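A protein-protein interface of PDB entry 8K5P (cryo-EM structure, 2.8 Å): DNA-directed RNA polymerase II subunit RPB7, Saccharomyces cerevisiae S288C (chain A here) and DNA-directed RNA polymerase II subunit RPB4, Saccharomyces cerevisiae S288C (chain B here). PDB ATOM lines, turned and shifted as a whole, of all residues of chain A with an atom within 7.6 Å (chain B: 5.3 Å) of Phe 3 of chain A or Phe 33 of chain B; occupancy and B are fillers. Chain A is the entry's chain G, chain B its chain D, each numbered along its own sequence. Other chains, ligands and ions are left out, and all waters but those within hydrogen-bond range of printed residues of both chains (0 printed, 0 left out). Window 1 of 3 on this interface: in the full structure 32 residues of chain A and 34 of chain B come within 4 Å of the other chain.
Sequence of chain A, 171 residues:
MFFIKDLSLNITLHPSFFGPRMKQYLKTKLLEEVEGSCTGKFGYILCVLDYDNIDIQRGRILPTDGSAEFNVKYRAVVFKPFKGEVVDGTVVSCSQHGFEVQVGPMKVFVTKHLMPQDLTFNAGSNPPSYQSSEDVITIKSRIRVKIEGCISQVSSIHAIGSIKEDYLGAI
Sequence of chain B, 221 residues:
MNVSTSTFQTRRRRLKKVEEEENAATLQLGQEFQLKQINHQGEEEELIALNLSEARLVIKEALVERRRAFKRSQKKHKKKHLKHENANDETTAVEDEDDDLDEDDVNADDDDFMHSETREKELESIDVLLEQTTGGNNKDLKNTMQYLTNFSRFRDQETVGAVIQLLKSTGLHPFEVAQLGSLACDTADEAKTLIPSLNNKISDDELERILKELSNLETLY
The side-chain amide nitrogen (NE2) of Gln 31 of chain B sits close to the side-chain amino group (NZ) of Lys 41 of chain A (3.2 Å).
NZ of Lys 5 of chain A is in salt-bridge range of OE1 of Glu 32 of chain B.
The backbone carbonyl oxygen of Leu 50 of chain B is in hydrogen-bond range of the backbone NH of Met 1 of chain A, 2.8 Å away.
OE1 of Gln 34 of chain B lies close to O of Gln 31 of chain B.
O of Glu 32 of chain B lies within hydrogen-bond range of NE2 of Gln 37 of chain B.
The backbone carbonyl oxygen (O) of Gln 34 of chain B sits at hydrogen-bond distance from the side-chain amide nitrogen (NE2) of Gln 37 of chain B (2.7 Å).
The backbone carbonyl oxygen of Phe 3 of chain A is in hydrogen-bond range of the backbone NH of Val 78 of chain A, at 3.0 Å.
The backbone carbonyl oxygen of Gly 40 of chain A sits at hydrogen-bond distance from the side-chain amino group of Lys 80 of chain A (3.4 Å).
The backbone carbonyl oxygen of Lys 41 of chain A is in hydrogen-bond range of the side-chain amino group of Lys 80 of chain A (2.6 Å).
Leu 50 of chain B touches Phe 2 of chain A.
CD2 of Phe 3 of chain A touches CE2 of Phe 33 of chain B, at 3.4 Å.
Phe 3 of chain A touches Ile 48 of chain B (CA to CD1, 3.9 Å).
Ile 4 of chain A touches Ile 48 of chain B (N to CD1, 3.6 Å).
Lys 5 of chain A touches Gln 37 of chain B (NZ to NE2, 3.9 Å).
CE of Lys 41 of chain A touches CB of Glu 32 of chain B, 3.7 Å away.
CE1 of Phe 42 of chain A touches OE2 of Glu 32 of chain B, 3.2 Å away.
CZ of Phe 33 of chain B touches CD of Lys 80 of chain A (3.6 Å).
Phe 82 of chain A touches Leu 29 of chain B.
Of chain B, only Phe 33 (3.4 Å) and Ile 48 (3.9 Å) come within 4 Å of Phe 3 of chain A.
Phe 33 of chain B touches just these residues of chain A: Phe 3 (3.4 Å) and Lys 80 (3.6 Å).
Of the printed residues of chain B, Phe 82 of chain A touches Leu 29 (3.5 Å).
Of the printed residues of chain B, Ile 4 of chain A touches Ile 48 (3.6 Å).
Of the printed residues of chain A, Ile 48 of chain B touches Phe 3 and Ile 4.
Ile 45 of chain A touches none of the printed residues of chain B.
Gln 34 of chain B touches none of the printed residues of chain A.
The nearest residue of chain B that does not touch Phe 3 of chain A is Phe 175 of chain B (4.1 Å).
Of the 12 printed residues of chain B, 7 touch a printed residue of chain A.
Printed residues of chain B that touch a printed residue of chain A: Leu 29, Gln 31, Glu 32, Phe 33, Gln 37, Ile 48 and Leu 50.
Hydrophobic or aromatic side chains of chain B within 4 Å of the printed part of chain A: Leu 29, Phe 33, Ile 48 and Leu 50.
Of the 20 printed residues of chain A, 9 touch a printed residue of chain B.
Printed residues of chain A that touch a printed residue of chain B: Met 1, Phe 2, Phe 3, Ile 4, Lys 5, Lys 41, Phe 42, Lys 80 and Phe 82.
Hydrophobic or aromatic side chains of chain A within 4 Å of the printed part of chain B: Phe 2, Phe 3, Ile 4, Phe 42 and Phe 82.
Along chain A the printed residues that touch a printed residue of chain B span positions 1 to 82.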
ATOM      1  N   MET A   1      -9.379   4.569 -28.299  1.00  0.00           N
ATOM      2  CA  MET A   1      -8.507   4.345 -27.152  1.00  0.00           C
ATOM      3  C   MET A   1      -7.055   4.407 -27.614  1.00  0.00           C
ATOM      4  O   MET A   1      -6.182   4.859 -26.871  1.00  0.00           O
ATOM      5  CB  MET A   1      -8.873   3.010 -26.469  1.00  0.00           C
ATOM      6  CG  MET A   1      -7.836   2.289 -25.574  1.00  0.00           C
ATOM      7  SD  MET A   1      -6.221   1.816 -26.234  1.00  0.00           S
ATOM      8  CE  MET A   1      -6.735   0.698 -27.534  1.00  0.00           C
ATOM      9  N   PHE A   2      -6.802   3.959 -28.842  1.00  0.00           N
ATOM     10  CA  PHE A   2      -5.473   4.100 -29.422  1.00  0.00           C
ATOM     11  C   PHE A   2      -5.132   5.579 -29.561  1.00  0.00           C
ATOM     12  O   PHE A   2      -6.010   6.417 -29.782  1.00  0.00           O
ATOM     13  CB  PHE A   2      -5.403   3.416 -30.788  1.00  0.00           C
ATOM     14  CG  PHE A   2      -5.559   1.923 -30.736  1.00  0.00           C
ATOM     15  CD1 PHE A   2      -4.519   1.117 -30.309  1.00  0.00           C
ATOM     16  CD2 PHE A   2      -6.744   1.326 -31.132  1.00  0.00           C
ATOM     17  CE1 PHE A   2      -4.662  -0.258 -30.271  1.00  0.00           C
ATOM     18  CE2 PHE A   2      -6.892  -0.047 -31.095  1.00  0.00           C
ATOM     19  CZ  PHE A   2      -5.849  -0.839 -30.662  1.00  0.00           C
ATOM     20  N   PHE A   3      -3.852   5.904 -29.419  1.00  0.00           N
ATOM     21  CA  PHE A   3      -3.407   7.287 -29.406  1.00  0.00           C
ATOM     22  C   PHE A   3      -2.449   7.559 -30.558  1.00  0.00           C
ATOM     23  O   PHE A   3      -1.687   6.684 -30.979  1.00  0.00           O
ATOM     24  CB  PHE A   3      -2.731   7.637 -28.076  1.00  0.00           C
ATOM     25  CG  PHE A   3      -3.625   7.467 -26.883  1.00  0.00           C
ATOM     26  CD1 PHE A   3      -4.762   8.244 -26.739  1.00  0.00           C
ATOM     27  CD2 PHE A   3      -3.333   6.528 -25.909  1.00  0.00           C
ATOM     28  CE1 PHE A   3      -5.589   8.091 -25.644  1.00  0.00           C
ATOM     29  CE2 PHE A   3      -4.155   6.370 -24.811  1.00  0.00           C
ATOM     30  CZ  PHE A   3      -5.286   7.152 -24.679  1.00  0.00           C
ATOM     31  N   ILE A   4      -2.506   8.787 -31.067  1.00  0.00           N
ATOM     32  CA  ILE A   4      -1.584   9.280 -32.083  1.00  0.00           C
ATOM     33  C   ILE A   4      -0.666  10.289 -31.409  1.00  0.00           C
ATOM     34  O   ILE A   4      -1.123  11.345 -30.953  1.00  0.00           O
ATOM     35  CB  ILE A   4      -2.327   9.917 -33.268  1.00  0.00           C
ATOM     36  CG1 ILE A   4      -3.130   8.869 -34.044  1.00  0.00           C
ATOM     37  CG2 ILE A   4      -1.346  10.622 -34.189  1.00  0.00           C
ATOM     38  CD1 ILE A   4      -2.492   7.500 -34.090  1.00  0.00           C
ATOM     39  N   LYS A   5       0.620   9.970 -31.344  1.00  0.00           N
ATOM     40  CA  LYS A   5       1.595  10.791 -30.641  1.00  0.00           C
ATOM     41  C   LYS A   5       2.662  11.285 -31.615  1.00  0.00           C
ATOM     42  O   LYS A   5       2.612  11.024 -32.819  1.00  0.00           O
ATOM     43  CB  LYS A   5       2.224  10.014 -29.482  1.00  0.00           C
ATOM     44  CG  LYS A   5       1.219   9.530 -28.450  1.00  0.00           C
ATOM     45  CD  LYS A   5       1.912   9.037 -27.191  1.00  0.00           C
ATOM     46  CE  LYS A   5       2.770  10.127 -26.574  1.00  0.00           C
ATOM     47  NZ  LYS A   5       1.978  11.350 -26.266  1.00  0.00           N
ATOM     48  N   ASP A   6       3.636  12.008 -31.070  1.00  0.00           N
ATOM     49  CA  ASP A   6       4.718  12.634 -31.826  1.00  0.00           C
ATOM     50  C   ASP A   6       6.067  12.210 -31.261  1.00  0.00           C
ATOM     51  O   ASP A   6       6.937  13.032 -30.966  1.00  0.00           O
ATOM     52  CB  ASP A   6       4.576  14.153 -31.824  1.00  0.00           C
ATOM     53  CG  ASP A   6       3.476  14.637 -32.747  1.00  0.00           C
ATOM     54  OD1 ASP A   6       2.966  13.822 -33.545  1.00  0.00           O
ATOM     55  OD2 ASP A   6       3.122  15.833 -32.677  1.00  0.00           O
ATOM     56  N   LEU A   7       6.241  10.902 -31.089  1.00  0.00           N
ATOM     57  CA  LEU A   7       7.443  10.351 -30.481  1.00  0.00           C
ATOM     58  C   LEU A   7       8.683  10.704 -31.303  1.00  0.00           C
ATOM     59  O   LEU A   7       8.606  11.193 -32.434  1.00  0.00           O
ATOM     60  CB  LEU A   7       7.331   8.831 -30.348  1.00  0.00           C
ATOM     61  CG  LEU A   7       6.048   8.170 -29.830  1.00  0.00           C
ATOM     62  CD1 LEU A   7       4.981   8.058 -30.911  1.00  0.00           C
ATOM     63  CD2 LEU A   7       6.366   6.800 -29.264  1.00  0.00           C
ATOM     64  N   GLY A  40       8.122   0.075 -22.804  1.00  0.00           N
ATOM     65  CA  GLY A  40       7.375   0.150 -21.558  1.00  0.00           C
ATOM     66  C   GLY A  40       6.647   1.468 -21.381  1.00  0.00           C
ATOM     67  O   GLY A  40       5.504   1.498 -20.916  1.00  0.00           O
ATOM     68  N   LYS A  41       7.299   2.576 -21.741  1.00  0.00           N
ATOM     69  CA  LYS A  41       6.699   3.892 -21.540  1.00  0.00           C
ATOM     70  C   LYS A  41       5.451   4.079 -22.394  1.00  0.00           C
ATOM     71  O   LYS A  41       4.446   4.623 -21.923  1.00  0.00           O
ATOM     72  CB  LYS A  41       7.725   4.983 -21.845  1.00  0.00           C
ATOM     73  CG  LYS A  41       7.196   6.400 -21.692  1.00  0.00           C
ATOM     74  CD  LYS A  41       6.647   6.640 -20.295  1.00  0.00           C
ATOM     75  CE  LYS A  41       5.331   7.400 -20.346  1.00  0.00           C
ATOM     76  NZ  LYS A  41       4.738   7.580 -18.993  1.00  0.00           N
ATOM     77  N   PHE A  42       5.492   3.633 -23.647  1.00  0.00           N
ATOM     78  CA  PHE A  42       4.411   3.865 -24.597  1.00  0.00           C
ATOM     79  C   PHE A  42       3.589   2.618 -24.888  1.00  0.00           C
ATOM     80  O   PHE A  42       2.363   2.639 -24.742  1.00  0.00           O
ATOM     81  CB  PHE A  42       4.991   4.427 -25.902  1.00  0.00           C
ATOM     82  CG  PHE A  42       5.799   5.677 -25.711  1.00  0.00           C
ATOM     83  CD1 PHE A  42       5.229   6.805 -25.146  1.00  0.00           C
ATOM     84  CD2 PHE A  42       7.135   5.715 -26.073  1.00  0.00           C
ATOM     85  CE1 PHE A  42       5.972   7.956 -24.964  1.00  0.00           C
ATOM     86  CE2 PHE A  42       7.882   6.864 -25.894  1.00  0.00           C
ATOM     87  CZ  PHE A  42       7.300   7.984 -25.337  1.00  0.00           C
ATOM     88  N   GLY A  43       4.231   1.528 -25.298  1.00  0.00           N
ATOM     89  CA  GLY A  43       3.514   0.307 -25.609  1.00  0.00           C
ATOM     90  C   GLY A  43       3.934  -0.313 -26.924  1.00  0.00           C
ATOM     91  O   GLY A  43       5.115  -0.609 -27.130  1.00  0.00           O
ATOM     92  N   TYR A  44       2.974  -0.517 -27.823  1.00  0.00           N
ATOM     93  CA  TYR A  44       3.230  -1.094 -29.135  1.00  0.00           C
ATOM     94  C   TYR A  44       3.121  -0.016 -30.201  1.00  0.00           C
ATOM     95  O   TYR A  44       2.144   0.741 -30.228  1.00  0.00           O
ATOM     96  CB  TYR A  44       2.248  -2.227 -29.445  1.00  0.00           C
ATOM     97  CG  TYR A  44       2.182  -3.305 -28.390  1.00  0.00           C
ATOM     98  CD1 TYR A  44       1.166  -3.319 -27.447  1.00  0.00           C
ATOM     99  CD2 TYR A  44       3.131  -4.317 -28.347  1.00  0.00           C
ATOM    100  CE1 TYR A  44       1.099  -4.306 -26.486  1.00  0.00           C
ATOM    101  CE2 TYR A  44       3.073  -5.310 -27.390  1.00  0.00           C
ATOM    102  CZ  TYR A  44       2.056  -5.299 -26.460  1.00  0.00           C
ATOM    103  OH  TYR A  44       1.994  -6.285 -25.504  1.00  0.00           O
ATOM    104  N   ILE A  45       4.119   0.050 -31.074  1.00  0.00           N
ATOM    105  CA  ILE A  45       4.086   0.928 -32.241  1.00  0.00           C
ATOM    106  C   ILE A  45       3.580   0.061 -33.389  1.00  0.00           C
ATOM    107  O   ILE A  45       4.342  -0.648 -34.049  1.00  0.00           O
ATOM    108  CB  ILE A  45       5.452   1.548 -32.533  1.00  0.00           C
ATOM    109  CG1 ILE A  45       5.925   2.394 -31.347  1.00  0.00           C
ATOM    110  CG2 ILE A  45       5.392   2.399 -33.792  1.00  0.00           C
ATOM    111  CD1 ILE A  45       4.839   3.247 -30.720  1.00  0.00           C
ATOM    112  N   LEU A  46       2.267   0.110 -33.621  1.00  0.00           N
ATOM    113  CA  LEU A  46       1.653  -0.768 -34.612  1.00  0.00           C
ATOM    114  C   LEU A  46       2.124  -0.430 -36.021  1.00  0.00           C
ATOM    115  O   LEU A  46       2.556  -1.315 -36.770  1.00  0.00           O
ATOM    116  CB  LEU A  46       0.128  -0.682 -34.520  1.00  0.00           C
ATOM    117  CG  LEU A  46      -0.546  -1.265 -33.276  1.00  0.00           C
ATOM    118  CD1 LEU A  46       0.156  -2.537 -32.819  1.00  0.00           C
ATOM    119  CD2 LEU A  46      -0.613  -0.242 -32.149  1.00  0.00           C
ATOM    120  N   ALA A  76       3.147   8.021 -35.010  1.00  0.00           N
ATOM    121  CA  ALA A  76       2.694   6.655 -35.224  1.00  0.00           C
ATOM    122  C   ALA A  76       1.591   6.314 -34.235  1.00  0.00           C
ATOM    123  O   ALA A  76       1.373   7.019 -33.245  1.00  0.00           O
ATOM    124  CB  ALA A  76       3.850   5.657 -35.089  1.00  0.00           C
ATOM    125  N   VAL A  77       0.894   5.218 -34.521  1.00  0.00           N
ATOM    126  CA  VAL A  77      -0.163   4.723 -33.645  1.00  0.00           C
ATOM    127  C   VAL A  77       0.466   3.931 -32.508  1.00  0.00           C
ATOM    128  O   VAL A  77       1.281   3.029 -32.739  1.00  0.00           O
ATOM    129  CB  VAL A  77      -1.163   3.862 -34.432  1.00  0.00           C
ATOM    130  CG1 VAL A  77      -2.474   3.744 -33.673  1.00  0.00           C
ATOM    131  CG2 VAL A  77      -1.390   4.444 -35.818  1.00  0.00           C
ATOM    132  N   VAL A  78       0.089   4.262 -31.276  1.00  0.00           N
ATOM    133  CA  VAL A  78       0.634   3.627 -30.084  1.00  0.00           C
ATOM    134  C   VAL A  78      -0.507   3.004 -29.291  1.00  0.00           C
ATOM    135  O   VAL A  78      -1.577   3.605 -29.141  1.00  0.00           O
ATOM    136  CB  VAL A  78       1.433   4.627 -29.220  1.00  0.00           C
ATOM    137  CG1 VAL A  78       0.576   5.823 -28.833  1.00  0.00           C
ATOM    138  CG2 VAL A  78       1.995   3.940 -27.983  1.00  0.00           C
ATOM    139  N   PHE A  79      -0.284   1.784 -28.807  1.00  0.00           N
ATOM    140  CA  PHE A  79      -1.248   1.060 -27.988  1.00  0.00           C
ATOM    141  C   PHE A  79      -0.660   0.874 -26.597  1.00  0.00           C
ATOM    142  O   PHE A  79       0.430   0.311 -26.452  1.00  0.00           O
ATOM    143  CB  PHE A  79      -1.591  -0.293 -28.617  1.00  0.00           C
ATOM    144  CG  PHE A  79      -2.457  -1.169 -27.754  1.00  0.00           C
ATOM    145  CD1 PHE A  79      -3.507  -0.635 -27.025  1.00  0.00           C
ATOM    146  CD2 PHE A  79      -2.224  -2.530 -27.681  1.00  0.00           C
ATOM    147  CE1 PHE A  79      -4.302  -1.443 -26.234  1.00  0.00           C
ATOM    148  CE2 PHE A  79      -3.016  -3.342 -26.894  1.00  0.00           C
ATOM    149  CZ  PHE A  79      -4.056  -2.798 -26.169  1.00  0.00           C
ATOM    150  N   LYS A  80      -1.381   1.342 -25.581  1.00  0.00           N
ATOM    151  CA  LYS A  80      -0.949   1.231 -24.200  1.00  0.00           C
ATOM    152  C   LYS A  80      -1.993   0.471 -23.393  1.00  0.00           C
ATOM    153  O   LYS A  80      -3.187   0.795 -23.475  1.00  0.00           O
ATOM    154  CB  LYS A  80      -0.721   2.621 -23.584  1.00  0.00           C
ATOM    155  CG  LYS A  80       0.089   2.603 -22.299  1.00  0.00           C
ATOM    156  CD  LYS A  80       0.448   4.012 -21.854  1.00  0.00           C
ATOM    157  CE  LYS A  80       1.301   3.992 -20.596  1.00  0.00           C
ATOM    158  NZ  LYS A  80       2.573   3.245 -20.800  1.00  0.00           N
ATOM    159  N   PHE A  82      -2.642   0.618 -20.258  1.00  0.00           N
ATOM    160  CA  PHE A  82      -3.238   1.606 -19.365  1.00  0.00           C
ATOM    161  C   PHE A  82      -3.848   0.923 -18.142  1.00  0.00           C
ATOM    162  O   PHE A  82      -3.565  -0.250 -17.881  1.00  0.00           O
ATOM    163  CB  PHE A  82      -4.282   2.430 -20.124  1.00  0.00           C
ATOM    164  CG  PHE A  82      -4.195   3.906 -19.872  1.00  0.00           C
ATOM    165  CD1 PHE A  82      -3.368   4.698 -20.651  1.00  0.00           C
ATOM    166  CD2 PHE A  82      -4.945   4.505 -18.879  1.00  0.00           C
ATOM    167  CE1 PHE A  82      -3.281   6.058 -20.436  1.00  0.00           C
ATOM    168  CE2 PHE A  82      -4.862   5.866 -18.662  1.00  0.00           C
ATOM    169  CZ  PHE A  82      -4.029   6.641 -19.440  1.00  0.00           C
ATOM    170  N   LEU B  29      -5.304  11.342 -15.403  1.00  0.00           N
ATOM    171  CA  LEU B  29      -4.407  10.916 -16.468  1.00  0.00           C
ATOM    172  C   LEU B  29      -2.953  10.927 -16.004  1.00  0.00           C
ATOM    173  O   LEU B  29      -2.596  11.521 -14.982  1.00  0.00           O
ATOM    174  CB  LEU B  29      -4.567  11.818 -17.692  1.00  0.00           C
ATOM    175  CG  LEU B  29      -5.532  11.341 -18.778  1.00  0.00           C
ATOM    176  CD1 LEU B  29      -5.133   9.966 -19.282  1.00  0.00           C
ATOM    177  CD2 LEU B  29      -6.957  11.326 -18.256  1.00  0.00           C
ATOM    178  N   GLY B  30      -2.105  10.255 -16.783  1.00  0.00           N
ATOM    179  CA  GLY B  30      -0.700  10.145 -16.465  1.00  0.00           C
ATOM    180  C   GLY B  30       0.078  11.408 -16.782  1.00  0.00           C
ATOM    181  O   GLY B  30      -0.432  12.376 -17.346  1.00  0.00           O
ATOM    182  N   GLN B  31       1.357  11.386 -16.397  1.00  0.00           N
ATOM    183  CA  GLN B  31       2.212  12.552 -16.592  1.00  0.00           C
ATOM    184  C   GLN B  31       2.472  12.817 -18.072  1.00  0.00           C
ATOM    185  O   GLN B  31       2.505  13.975 -18.502  1.00  0.00           O
ATOM    186  CB  GLN B  31       3.531  12.364 -15.842  1.00  0.00           C
ATOM    187  CG  GLN B  31       4.134  10.976 -15.981  1.00  0.00           C
ATOM    188  CD  GLN B  31       5.226  10.918 -17.032  1.00  0.00           C
ATOM    189  OE1 GLN B  31       5.430  11.869 -17.785  1.00  0.00           O
ATOM    190  NE2 GLN B  31       5.936   9.797 -17.086  1.00  0.00           N
ATOM    191  N   GLU B  32       2.663  11.761 -18.862  1.00  0.00           N
ATOM    192  CA  GLU B  32       3.017  11.921 -20.266  1.00  0.00           C
ATOM    193  C   GLU B  32       1.806  11.949 -21.190  1.00  0.00           C
ATOM    194  O   GLU B  32       1.882  12.532 -22.278  1.00  0.00           O
ATOM    195  CB  GLU B  32       3.960  10.797 -20.704  1.00  0.00           C
ATOM    196  CG  GLU B  32       4.864  11.164 -21.868  1.00  0.00           C
ATOM    197  CD  GLU B  32       4.338  10.658 -23.195  1.00  0.00           C
ATOM    198  OE1 GLU B  32       3.277  10.000 -23.204  1.00  0.00           O
ATOM    199  OE2 GLU B  32       4.985  10.917 -24.231  1.00  0.00           O
ATOM    200  N   PHE B  33       0.693  11.338 -20.786  1.00  0.00           N
ATOM    201  CA  PHE B  33      -0.512  11.277 -21.605  1.00  0.00           C
ATOM    202  C   PHE B  33      -1.520  12.358 -21.228  1.00  0.00           C
ATOM    203  O   PHE B  33      -2.731  12.158 -21.375  1.00  0.00           O
ATOM    204  CB  PHE B  33      -1.149   9.893 -21.506  1.00  0.00           C
ATOM    205  CG  PHE B  33      -0.475   8.855 -22.357  1.00  0.00           C
ATOM    206  CD1 PHE B  33       0.759   8.340 -21.997  1.00  0.00           C
ATOM    207  CD2 PHE B  33      -1.072   8.397 -23.519  1.00  0.00           C
ATOM    208  CE1 PHE B  33       1.383   7.386 -22.777  1.00  0.00           C
ATOM    209  CE2 PHE B  33      -0.451   7.443 -24.304  1.00  0.00           C
ATOM    210  CZ  PHE B  33       0.777   6.938 -23.932  1.00  0.00           C
ATOM    211  N   GLN B  34      -1.042  13.500 -20.745  1.00  0.00           N
ATOM    212  CA  GLN B  34      -1.919  14.587 -20.341  1.00  0.00           C
ATOM    213  C   GLN B  34      -2.465  15.320 -21.566  1.00  0.00           C
ATOM    214  O   GLN B  34      -1.987  15.158 -22.692  1.00  0.00           O
ATOM    215  CB  GLN B  34      -1.175  15.556 -19.421  1.00  0.00           C
ATOM    216  CG  GLN B  34      -0.428  16.669 -20.143  1.00  0.00           C
ATOM    217  CD  GLN B  34       0.652  16.148 -21.072  1.00  0.00           C
ATOM    218  OE1 GLN B  34       1.306  15.146 -20.783  1.00  0.00           O
ATOM    219  NE2 GLN B  34       0.845  16.829 -22.196  1.00  0.00           N
ATOM    220  N   LEU B  35      -3.489  16.137 -21.330  1.00  0.00           N
ATOM    221  CA  LEU B  35      -4.103  16.903 -22.403  1.00  0.00           C
ATOM    222  C   LEU B  35      -3.170  18.017 -22.873  1.00  0.00           C
ATOM    223  O   LEU B  35      -2.233  18.418 -22.175  1.00  0.00           O
ATOM    224  CB  LEU B  35      -5.435  17.493 -21.942  1.00  0.00           C
ATOM    225  CG  LEU B  35      -6.526  17.638 -23.005  1.00  0.00           C
ATOM    226  CD1 LEU B  35      -6.738  16.324 -23.739  1.00  0.00           C
ATOM    227  CD2 LEU B  35      -7.825  18.122 -22.378  1.00  0.00           C
ATOM    228  N   GLN B  37      -0.955  18.169 -25.631  1.00  0.00           N
ATOM    229  CA  GLN B  37       0.400  17.707 -25.879  1.00  0.00           C
ATOM    230  C   GLN B  37       1.167  18.722 -26.723  1.00  0.00           C
ATOM    231  O   GLN B  37       0.589  19.564 -27.415  1.00  0.00           O
ATOM    232  CB  GLN B  37       0.384  16.347 -26.579  1.00  0.00           C
ATOM    233  CG  GLN B  37      -0.474  15.302 -25.885  1.00  0.00           C
ATOM    234  CD  GLN B  37       0.274  14.560 -24.795  1.00  0.00           C
ATOM    235  OE1 GLN B  37       1.431  14.864 -24.502  1.00  0.00           O
ATOM    236  NE2 GLN B  37      -0.386  13.583 -24.185  1.00  0.00           N
ATOM    237  N   LEU B  47      -5.003  16.427 -27.360  1.00  0.00           N
ATOM    238  CA  LEU B  47      -4.987  14.995 -27.619  1.00  0.00           C
ATOM    239  C   LEU B  47      -6.103  14.619 -28.585  1.00  0.00           C
ATOM    240  O   LEU B  47      -7.205  15.173 -28.534  1.00  0.00           O
ATOM    241  CB  LEU B  47      -5.133  14.214 -26.314  1.00  0.00           C
ATOM    242  CG  LEU B  47      -4.812  12.720 -26.373  1.00  0.00           C
ATOM    243  CD1 LEU B  47      -3.526  12.474 -27.144  1.00  0.00           C
ATOM    244  CD2 LEU B  47      -4.720  12.137 -24.971  1.00  0.00           C
ATOM    245  N   ILE B  48      -5.809  13.668 -29.475  1.00  0.00           N
ATOM    246  CA  ILE B  48      -6.789  13.276 -30.480  1.00  0.00           C
ATOM    247  C   ILE B  48      -7.939  12.498 -29.844  1.00  0.00           C
ATOM    248  O   ILE B  48      -7.843  11.975 -28.727  1.00  0.00           O
ATOM    249  CB  ILE B  48      -6.121  12.486 -31.623  1.00  0.00           C
ATOM    250  CG1 ILE B  48      -5.099  11.442 -31.124  1.00  0.00           C
ATOM    251  CG2 ILE B  48      -5.459  13.438 -32.609  1.00  0.00           C
ATOM    252  CD1 ILE B  48      -5.585  10.390 -30.142  1.00  0.00           C
ATOM    253  N   LEU B  50      -9.683   9.435 -30.905  1.00  0.00           N
ATOM    254  CA  LEU B  50      -9.588   8.313 -31.828  1.00  0.00           C
ATOM    255  C   LEU B  50     -10.313   7.123 -31.212  1.00  0.00           C
ATOM    256  O   LEU B  50      -9.971   6.690 -30.106  1.00  0.00           O
ATOM    257  CB  LEU B  50      -8.120   7.984 -32.115  1.00  0.00           C
ATOM    258  CG  LEU B  50      -7.680   6.789 -32.973  1.00  0.00           C
ATOM    259  CD1 LEU B  50      -7.759   5.459 -32.244  1.00  0.00           C
ATOM    260  CD2 LEU B  50      -8.459   6.740 -34.273  1.00  0.00           C
ATOM    261  N   PHE B 175     -10.673  10.472 -24.216  1.00  0.00           N
ATOM    262  CA  PHE B 175     -10.639   9.094 -23.737  1.00  0.00           C
ATOM    263  C   PHE B 175     -12.049   8.567 -23.497  1.00  0.00           C
ATOM    264  O   PHE B 175     -12.358   7.420 -23.842  1.00  0.00           O
ATOM    265  CB  PHE B 175      -9.787   9.010 -22.465  1.00  0.00           C
ATOM    266  CG  PHE B 175      -9.648   7.617 -21.899  1.00  0.00           C
ATOM    267  CD1 PHE B 175      -8.450   6.933 -22.015  1.00  0.00           C
ATOM    268  CD2 PHE B 175     -10.686   7.018 -21.198  1.00  0.00           C
ATOM    269  CE1 PHE B 175      -8.306   5.663 -21.489  1.00  0.00           C
ATOM    270  CE2 PHE B 175     -10.546   5.749 -20.672  1.00  0.00           C
ATOM    271  CZ  PHE B 175      -9.354   5.073 -20.814  1.00  0.00           C
